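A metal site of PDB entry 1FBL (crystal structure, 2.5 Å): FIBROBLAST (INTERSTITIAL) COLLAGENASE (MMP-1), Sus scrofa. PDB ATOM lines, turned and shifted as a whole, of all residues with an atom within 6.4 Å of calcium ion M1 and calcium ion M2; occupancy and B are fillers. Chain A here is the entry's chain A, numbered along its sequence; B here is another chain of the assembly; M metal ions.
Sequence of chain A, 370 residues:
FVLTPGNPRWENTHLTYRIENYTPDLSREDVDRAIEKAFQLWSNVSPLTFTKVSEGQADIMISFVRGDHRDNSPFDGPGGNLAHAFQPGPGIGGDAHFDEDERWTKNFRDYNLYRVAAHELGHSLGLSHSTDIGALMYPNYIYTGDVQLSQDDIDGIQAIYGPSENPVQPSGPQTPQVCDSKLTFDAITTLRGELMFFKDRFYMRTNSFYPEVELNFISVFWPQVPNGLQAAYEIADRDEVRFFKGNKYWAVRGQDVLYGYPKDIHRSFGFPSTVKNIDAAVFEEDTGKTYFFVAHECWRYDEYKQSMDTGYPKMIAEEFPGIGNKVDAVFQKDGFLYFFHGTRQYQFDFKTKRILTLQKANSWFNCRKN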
ATOM      1  N   THR A  23      11.434 -16.737  11.622  1.00  0.00           N
ATOM      2  CA  THR A  23       9.983 -16.975  11.665  1.00  0.00           C
ATOM      3  C   THR A  23       9.322 -16.794  10.308  1.00  0.00           C
ATOM      4  O   THR A  23       9.519 -15.759   9.684  1.00  0.00           O
ATOM      5  CB  THR A  23       9.290 -15.995  12.650  1.00  0.00           C
ATOM      6  OG1 THR A  23       7.871 -16.258  12.687  1.00  0.00           O
ATOM      7  CG2 THR A  23       9.528 -14.557  12.251  1.00  0.00           C
ATOM      8  N   PRO A  24       8.503 -17.782   9.842  1.00  0.00           N
ATOM      9  CA  PRO A  24       7.815 -17.649   8.541  1.00  0.00           C
ATOM     10  C   PRO A  24       6.802 -16.490   8.533  1.00  0.00           C
ATOM     11  O   PRO A  24       6.247 -16.181   7.495  1.00  0.00           O
ATOM     12  CB  PRO A  24       7.074 -18.980   8.407  1.00  0.00           C
ATOM     13  CG  PRO A  24       7.810 -19.912   9.257  1.00  0.00           C
ATOM     14  CD  PRO A  24       8.232 -19.099  10.444  1.00  0.00           C
ATOM     15  N   ASP A  25       6.523 -15.913   9.701  1.00  0.00           N
ATOM     16  CA  ASP A  25       5.578 -14.798   9.829  1.00  0.00           C
ATOM     17  C   ASP A  25       6.096 -13.538   9.096  1.00  0.00           C
ATOM     18  O   ASP A  25       5.334 -12.819   8.484  1.00  0.00           O
ATOM     19  CB  ASP A  25       5.300 -14.476  11.325  1.00  0.00           C
ATOM     20  CG  ASP A  25       4.557 -15.593  12.044  1.00  0.00           C
ATOM     21  OD1 ASP A  25       3.997 -16.462  11.389  1.00  0.00           O
ATOM     22  OD2 ASP A  25       4.556 -15.626  13.285  1.00  0.00           O
ATOM     23  N   ARG A  66       8.830 -23.185  20.363  1.00  0.00           N
ATOM     24  CA  ARG A  66       7.457 -23.347  20.807  1.00  0.00           C
ATOM     25  C   ARG A  66       7.364 -24.606  21.640  1.00  0.00           C
ATOM     26  O   ARG A  66       8.199 -25.512  21.536  1.00  0.00           O
ATOM     27  CB  ARG A  66       6.479 -23.415  19.645  1.00  0.00           C
ATOM     28  CG  ARG A  66       6.643 -24.569  18.745  1.00  0.00           C
ATOM     29  CD  ARG A  66       5.511 -24.612  17.755  1.00  0.00           C
ATOM     30  NE  ARG A  66       5.961 -24.318  16.414  1.00  0.00           N
ATOM     31  CZ  ARG A  66       5.147 -23.951  15.419  1.00  0.00           C
ATOM     32  NH1 ARG A  66       3.844 -23.855  15.639  1.00  0.00           N
ATOM     33  NH2 ARG A  66       5.641 -23.646  14.228  1.00  0.00           N
ATOM     34  N   PHE A  75       7.147 -23.188  26.351  1.00  0.00           N
ATOM     35  CA  PHE A  75       6.139 -22.198  26.021  1.00  0.00           C
ATOM     36  C   PHE A  75       4.725 -22.782  26.145  1.00  0.00           C
ATOM     37  O   PHE A  75       4.539 -23.971  26.442  1.00  0.00           O
ATOM     38  CB  PHE A  75       6.401 -21.541  24.658  1.00  0.00           C
ATOM     39  CG  PHE A  75       7.470 -20.479  24.701  1.00  0.00           C
ATOM     40  CD1 PHE A  75       7.461 -19.500  25.677  1.00  0.00           C
ATOM     41  CD2 PHE A  75       8.535 -20.501  23.814  1.00  0.00           C
ATOM     42  CE1 PHE A  75       8.508 -18.575  25.760  1.00  0.00           C
ATOM     43  CE2 PHE A  75       9.573 -19.568  23.906  1.00  0.00           C
ATOM     44  CZ  PHE A  75       9.559 -18.622  24.860  1.00  0.00           C
ATOM     45  N   ASP A  76       3.721 -21.947  25.896  1.00  0.00           N
ATOM     46  CA  ASP A  76       2.320 -22.269  26.188  1.00  0.00           C
ATOM     47  C   ASP A  76       1.367 -22.186  24.998  1.00  0.00           C
ATOM     48  O   ASP A  76       0.147 -22.220  25.173  1.00  0.00           O
ATOM     49  CB  ASP A  76       1.816 -21.335  27.319  1.00  0.00           C
ATOM     50  CG  ASP A  76       1.941 -19.806  26.990  1.00  0.00           C
ATOM     51  OD1 ASP A  76       2.682 -19.379  26.061  1.00  0.00           O
ATOM     52  OD2 ASP A  76       1.301 -19.023  27.716  1.00  0.00           O
ATOM     53  N   GLY A  77       1.924 -22.073  23.803  1.00  0.00           N
ATOM     54  CA  GLY A  77       1.078 -21.947  22.651  1.00  0.00           C
ATOM     55  C   GLY A  77       0.780 -20.496  22.403  1.00  0.00           C
ATOM     56  O   GLY A  77       1.486 -19.603  22.941  1.00  0.00           O
ATOM     57  N   PRO A  78      -0.242 -20.212  21.574  1.00  0.00           N
ATOM     58  CA  PRO A  78      -0.696 -18.875  21.190  1.00  0.00           C
ATOM     59  C   PRO A  78      -1.055 -18.009  22.402  1.00  0.00           C
ATOM     60  O   PRO A  78      -1.773 -18.461  23.328  1.00  0.00           O
ATOM     61  CB  PRO A  78      -1.923 -19.176  20.327  1.00  0.00           C
ATOM     62  CG  PRO A  78      -1.695 -20.553  19.816  1.00  0.00           C
ATOM     63  CD  PRO A  78      -1.128 -21.239  21.003  1.00  0.00           C
ATOM     64  N   GLY A  79      -0.544 -16.769  22.384  1.00  0.00           N
ATOM     65  CA  GLY A  79      -0.752 -15.811  23.450  1.00  0.00           C
ATOM     66  C   GLY A  79      -0.028 -16.083  24.749  1.00  0.00           C
ATOM     67  O   GLY A  79       0.896 -16.924  24.815  1.00  0.00           O
ATOM     68  N   GLY A  80      -0.432 -15.348  25.773  1.00  0.00           N
ATOM     69  CA  GLY A  80       0.115 -15.486  27.096  1.00  0.00           C
ATOM     70  C   GLY A  80       1.588 -15.199  27.012  1.00  0.00           C
ATOM     71  O   GLY A  80       1.954 -14.149  26.524  1.00  0.00           O
ATOM     72  N   ASN A  81       2.398 -16.171  27.448  1.00  0.00           N
ATOM     73  CA  ASN A  81       3.858 -16.182  27.355  1.00  0.00           C
ATOM     74  C   ASN A  81       4.282 -16.055  25.869  1.00  0.00           C
ATOM     75  O   ASN A  81       3.903 -16.930  25.006  1.00  0.00           O
ATOM     76  CB  ASN A  81       4.352 -17.503  27.935  1.00  0.00           C
ATOM     77  CG  ASN A  81       5.791 -17.474  28.368  1.00  0.00           C
ATOM     78  OD1 ASN A  81       6.490 -16.453  28.268  1.00  0.00           O
ATOM     79  ND2 ASN A  81       6.249 -18.590  28.909  1.00  0.00           N
ATOM     80  N   LEU A  82       5.002 -14.951  25.595  1.00  0.00           N
ATOM     81  CA  LEU A  82       5.475 -14.575  24.254  1.00  0.00           C
ATOM     82  C   LEU A  82       6.932 -14.940  24.050  1.00  0.00           C
ATOM     83  O   LEU A  82       7.287 -15.482  23.008  1.00  0.00           O
ATOM     84  CB  LEU A  82       5.371 -13.047  24.029  1.00  0.00           C
ATOM     85  CG  LEU A  82       4.232 -12.081  24.429  1.00  0.00           C
ATOM     86  CD1 LEU A  82       4.432 -10.797  23.713  1.00  0.00           C
ATOM     87  CD2 LEU A  82       2.897 -12.648  24.056  1.00  0.00           C
ATOM     88  N   ALA A  83       7.782 -14.634  25.024  1.00  0.00           N
ATOM     89  CA  ALA A  83       9.211 -14.886  24.894  1.00  0.00           C
ATOM     90  C   ALA A  83       9.911 -14.897  26.230  1.00  0.00           C
ATOM     91  O   ALA A  83       9.299 -14.565  27.242  1.00  0.00           O
ATOM     92  CB  ALA A  83       9.831 -13.824  24.000  1.00  0.00           C
ATOM     93  N   ASP A  99       8.427 -17.475  21.316  1.00  0.00           N
ATOM     94  CA  ASP A  99       7.358 -18.480  21.035  1.00  0.00           C
ATOM     95  C   ASP A  99       6.714 -18.391  19.611  1.00  0.00           C
ATOM     96  O   ASP A  99       5.946 -17.481  19.325  1.00  0.00           O
ATOM     97  CB  ASP A  99       6.296 -18.367  22.125  1.00  0.00           C
ATOM     98  CG  ASP A  99       5.210 -19.396  22.022  1.00  0.00           C
ATOM     99  OD1 ASP A  99       5.313 -20.338  21.219  1.00  0.00           O
ATOM    100  OD2 ASP A  99       4.221 -19.264  22.770  1.00  0.00           O
ATOM    101  N   GLU A 100       6.944 -19.392  18.758  1.00  0.00           N
ATOM    102  CA  GLU A 100       6.555 -19.348  17.343  1.00  0.00           C
ATOM    103  C   GLU A 100       5.062 -19.465  17.083  1.00  0.00           C
ATOM    104  O   GLU A 100       4.565 -19.141  15.975  1.00  0.00           O
ATOM    105  CB  GLU A 100       7.307 -20.418  16.544  1.00  0.00           C
ATOM    106  CG  GLU A 100       7.061 -20.395  15.074  1.00  0.00           C
ATOM    107  CD  GLU A 100       7.484 -19.094  14.443  1.00  0.00           C
ATOM    108  OE1 GLU A 100       8.698 -18.928  14.291  1.00  0.00           O
ATOM    109  OE2 GLU A 100       6.609 -18.235  14.113  1.00  0.00           O
ATOM    110  N   ASP A 101       4.359 -19.921  18.132  1.00  0.00           N
ATOM    111  CA  ASP A 101       2.898 -20.004  18.167  1.00  0.00           C
ATOM    112  C   ASP A 101       2.305 -18.611  18.172  1.00  0.00           C
ATOM    113  O   ASP A 101       1.091 -18.476  18.071  1.00  0.00           O
ATOM    114  CB  ASP A 101       2.396 -20.728  19.414  1.00  0.00           C
ATOM    115  CG  ASP A 101       2.552 -22.248  19.352  1.00  0.00           C
ATOM    116  OD1 ASP A 101       2.394 -22.877  18.265  1.00  0.00           O
ATOM    117  OD2 ASP A 101       2.808 -22.823  20.431  1.00  0.00           O
ATOM    118  N   GLU A 102       3.148 -17.584  18.401  1.00  0.00           N
ATOM    119  CA  GLU A 102       2.741 -16.178  18.277  1.00  0.00           C
ATOM    120  C   GLU A 102       2.820 -15.669  16.815  1.00  0.00           C
ATOM    121  O   GLU A 102       3.722 -16.059  16.015  1.00  0.00           O
ATOM    122  CB  GLU A 102       3.587 -15.247  19.169  1.00  0.00           C
ATOM    123  CG  GLU A 102       3.702 -15.596  20.623  1.00  0.00           C
ATOM    124  CD  GLU A 102       2.375 -15.922  21.256  1.00  0.00           C
ATOM    125  OE1 GLU A 102       1.312 -15.593  20.670  1.00  0.00           O
ATOM    126  OE2 GLU A 102       2.378 -16.552  22.329  1.00  0.00           O
ATOM    127  N   ARG A 103       1.842 -14.863  16.425  1.00  0.00           N
ATOM    128  CA  ARG A 103       1.875 -14.206  15.113  1.00  0.00           C
ATOM    129  C   ARG A 103       2.846 -13.019  15.244  1.00  0.00           C
ATOM    130  O   ARG A 103       2.524 -12.002  15.884  1.00  0.00           O
ATOM    131  CB  ARG A 103       0.475 -13.724  14.734  1.00  0.00           C
ATOM    132  CG  ARG A 103       0.209 -13.606  13.239  1.00  0.00           C
ATOM    133  CD  ARG A 103       1.128 -12.628  12.573  1.00  0.00           C
ATOM    134  NE  ARG A 103       0.662 -12.306  11.234  1.00  0.00           N
ATOM    135  CZ  ARG A 103       1.051 -12.951  10.138  1.00  0.00           C
ATOM    136  NH1 ARG A 103       1.964 -13.910  10.198  1.00  0.00           N
ATOM    137  NH2 ARG A 103       0.452 -12.701   8.966  1.00  0.00           N
ATOM    138  N   TRP A 104       4.043 -13.165  14.698  1.00  0.00           N
ATOM    139  CA  TRP A 104       5.017 -12.096  14.804  1.00  0.00           C
ATOM    140  C   TRP A 104       4.735 -10.987  13.813  1.00  0.00           C
ATOM    141  O   TRP A 104       4.684 -11.232  12.611  1.00  0.00           O
ATOM    142  CB  TRP A 104       6.427 -12.684  14.666  1.00  0.00           C
ATOM    143  CG  TRP A 104       6.798 -13.530  15.913  1.00  0.00           C
ATOM    144  CD1 TRP A 104       7.005 -14.870  15.952  1.00  0.00           C
ATOM    145  CD2 TRP A 104       6.836 -13.072  17.286  1.00  0.00           C
ATOM    146  NE1 TRP A 104       7.153 -15.284  17.246  1.00  0.00           N
ATOM    147  CE2 TRP A 104       7.046 -14.202  18.079  1.00  0.00           C
ATOM    148  CE3 TRP A 104       6.712 -11.818  17.896  1.00  0.00           C
ATOM    149  CZ2 TRP A 104       7.134 -14.122  19.473  1.00  0.00           C
ATOM    150  CZ3 TRP A 104       6.796 -11.736  19.253  1.00  0.00           C
ATOM    151  CH2 TRP A 104       7.004 -12.883  20.034  1.00  0.00           C
ATOM    152  N   ASN B 140      -5.530 -18.307  27.652  1.00  0.00           N
ATOM    153  CA  ASN B 140      -5.075 -16.971  27.316  1.00  0.00           C
ATOM    154  C   ASN B 140      -6.114 -16.132  26.575  1.00  0.00           C
ATOM    155  O   ASN B 140      -6.918 -16.658  25.800  1.00  0.00           O
ATOM    156  CB  ASN B 140      -3.832 -17.036  26.434  1.00  0.00           C
ATOM    157  CG  ASN B 140      -2.683 -17.801  27.060  1.00  0.00           C
ATOM    158  OD1 ASN B 140      -1.847 -18.338  26.326  1.00  0.00           O
ATOM    159  ND2 ASN B 140      -2.576 -17.805  28.394  1.00  0.00           N
ATOM    160  N   ARG B 205      -1.961 -24.326   8.864  1.00  0.00           N
ATOM    161  CA  ARG B 205      -0.717 -24.034   8.176  1.00  0.00           C
ATOM    162  C   ARG B 205       0.197 -25.267   8.240  1.00  0.00           C
ATOM    163  O   ARG B 205       0.179 -25.997   9.232  1.00  0.00           O
ATOM    164  CB  ARG B 205      -0.068 -22.842   8.878  1.00  0.00           C
ATOM    165  CG  ARG B 205       1.197 -22.282   8.294  1.00  0.00           C
ATOM    166  CD  ARG B 205       1.480 -21.041   9.096  1.00  0.00           C
ATOM    167  NE  ARG B 205       2.656 -20.287   8.676  1.00  0.00           N
ATOM    168  CZ  ARG B 205       3.044 -19.153   9.239  1.00  0.00           C
ATOM    169  NH1 ARG B 205       2.356 -18.627  10.219  1.00  0.00           N
ATOM    170  NH2 ARG B 205       4.141 -18.545   8.850  1.00  0.00           N
ATOM    171  N   TYR B 210       7.223 -28.397   8.825  1.00  0.00           N
ATOM    172  CA  TYR B 210       6.403 -28.505  10.036  1.00  0.00           C
ATOM    173  C   TYR B 210       6.152 -29.883  10.703  1.00  0.00           C
ATOM    174  O   TYR B 210       5.524 -30.777  10.114  1.00  0.00           O
ATOM    175  CB  TYR B 210       5.035 -27.873   9.786  1.00  0.00           C
ATOM    176  CG  TYR B 210       5.020 -26.375   9.901  1.00  0.00           C
ATOM    177  CD1 TYR B 210       5.897 -25.601   9.150  1.00  0.00           C
ATOM    178  CD2 TYR B 210       4.109 -25.735  10.751  1.00  0.00           C
ATOM    179  CE1 TYR B 210       5.879 -24.232   9.221  1.00  0.00           C
ATOM    180  CE2 TYR B 210       4.061 -24.355  10.830  1.00  0.00           C
ATOM    181  CZ  TYR B 210       4.958 -23.601  10.069  1.00  0.00           C
ATOM    182  OH  TYR B 210       4.976 -22.232  10.149  1.00  0.00           O
ATOM    183  N   GLU B 214      -0.334 -26.255  12.151  1.00  0.00           N
ATOM    184  CA  GLU B 214      -0.577 -25.187  13.103  1.00  0.00           C
ATOM    185  C   GLU B 214      -2.021 -24.728  12.942  1.00  0.00           C
ATOM    186  O   GLU B 214      -2.410 -24.214  11.891  1.00  0.00           O
ATOM    187  CB  GLU B 214       0.379 -24.022  12.848  1.00  0.00           C
ATOM    188  CG  GLU B 214      -0.132 -22.705  13.417  1.00  0.00           C
ATOM    189  CD  GLU B 214       0.776 -21.534  13.093  1.00  0.00           C
ATOM    190  OE1 GLU B 214       1.969 -21.575  13.451  1.00  0.00           O
ATOM    191  OE2 GLU B 214       0.301 -20.562  12.462  1.00  0.00           O
ATOM    192  N   PHE B 221      -4.180 -14.124  12.220  1.00  0.00           N
ATOM    193  CA  PHE B 221      -3.183 -14.105  11.167  1.00  0.00           C
ATOM    194  C   PHE B 221      -3.304 -12.828  10.339  1.00  0.00           C
ATOM    195  O   PHE B 221      -2.323 -12.134  10.152  1.00  0.00           O
ATOM    196  CB  PHE B 221      -3.362 -15.307  10.253  1.00  0.00           C
ATOM    197  CG  PHE B 221      -2.092 -15.850   9.729  1.00  0.00           C
ATOM    198  CD1 PHE B 221      -1.153 -16.378  10.609  1.00  0.00           C
ATOM    199  CD2 PHE B 221      -1.746 -15.688   8.388  1.00  0.00           C
ATOM    200  CE1 PHE B 221       0.108 -16.723  10.175  1.00  0.00           C
ATOM    201  CE2 PHE B 221      -0.487 -16.023   7.923  1.00  0.00           C
ATOM    202  CZ  PHE B 221       0.444 -16.544   8.812  1.00  0.00           C
HETATM  203 CA    CA M   1       2.617 -18.059  24.001  1.00  0.00          CA
HETATM  204 CA    CA M   2       4.411 -17.860  14.236  1.00  0.00          CA
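Calcium ion M1 is bound by O of Asn 81, O of Gly 77, O of Gly 79, OE2 of Glu 102, OD2 of Asp 99 and OD1 of Asp 76. Calcium ion M1 has six donor atoms within binding distance.
The nearest printed residue that does not touch calcium ion M2 is Thr 23 (4.1 Å).
Within 4 Å of calcium ion M1: Asp 76, Gly 77, Gly 79, Asn 81, Asp 99 and Glu 102. The nearest printed residue that does not touch calcium ion M1 is Pro 78 (4.01 Å).
Calcium ion M2 is bound by O of Glu 100 (2.2 Å), OE2 of Glu 100 (2.2 Å), OD2 of Asp 25 (2.4 Å) and O of Glu 102 (2.6 Å).
The indole nitrogen (NE1) of Trp 104 is in hydrogen-bond range of the backbone carbonyl oxygen (O) of Asp 99 (3.3 Å). The side-chain carboxylate (OD1) of Asp 99 lies close to the backbone NH (N) of Asp 101 (3.3 Å). OD2 of Asp 25 sits close to N of Trp 104, at 2.9 Å. The backbone carbonyl oxygen (O) of Leu 82 is in hydrogen-bond range of the backbone NH (N) of Asp 99, at 2.9 Å. The backbone NH of Asp 25 sits close to the side-chain hydroxyl of Thr 23 (3.3 Å). The side-chain carboxylate (OD1) of Asp 25 lies within salt-bridge range of the guanidinium group (NH1) of Arg 205 of chain B, at 3.0 Å. The side-chain carboxylate of Asp 25 is in salt-bridge range of the guanidinium group of Arg 103, 3.5 Å away. The side-chain amide oxygen of Asn 140 of chain B sits close to the backbone carbonyl oxygen of Gly 79, at 3.4 Å.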
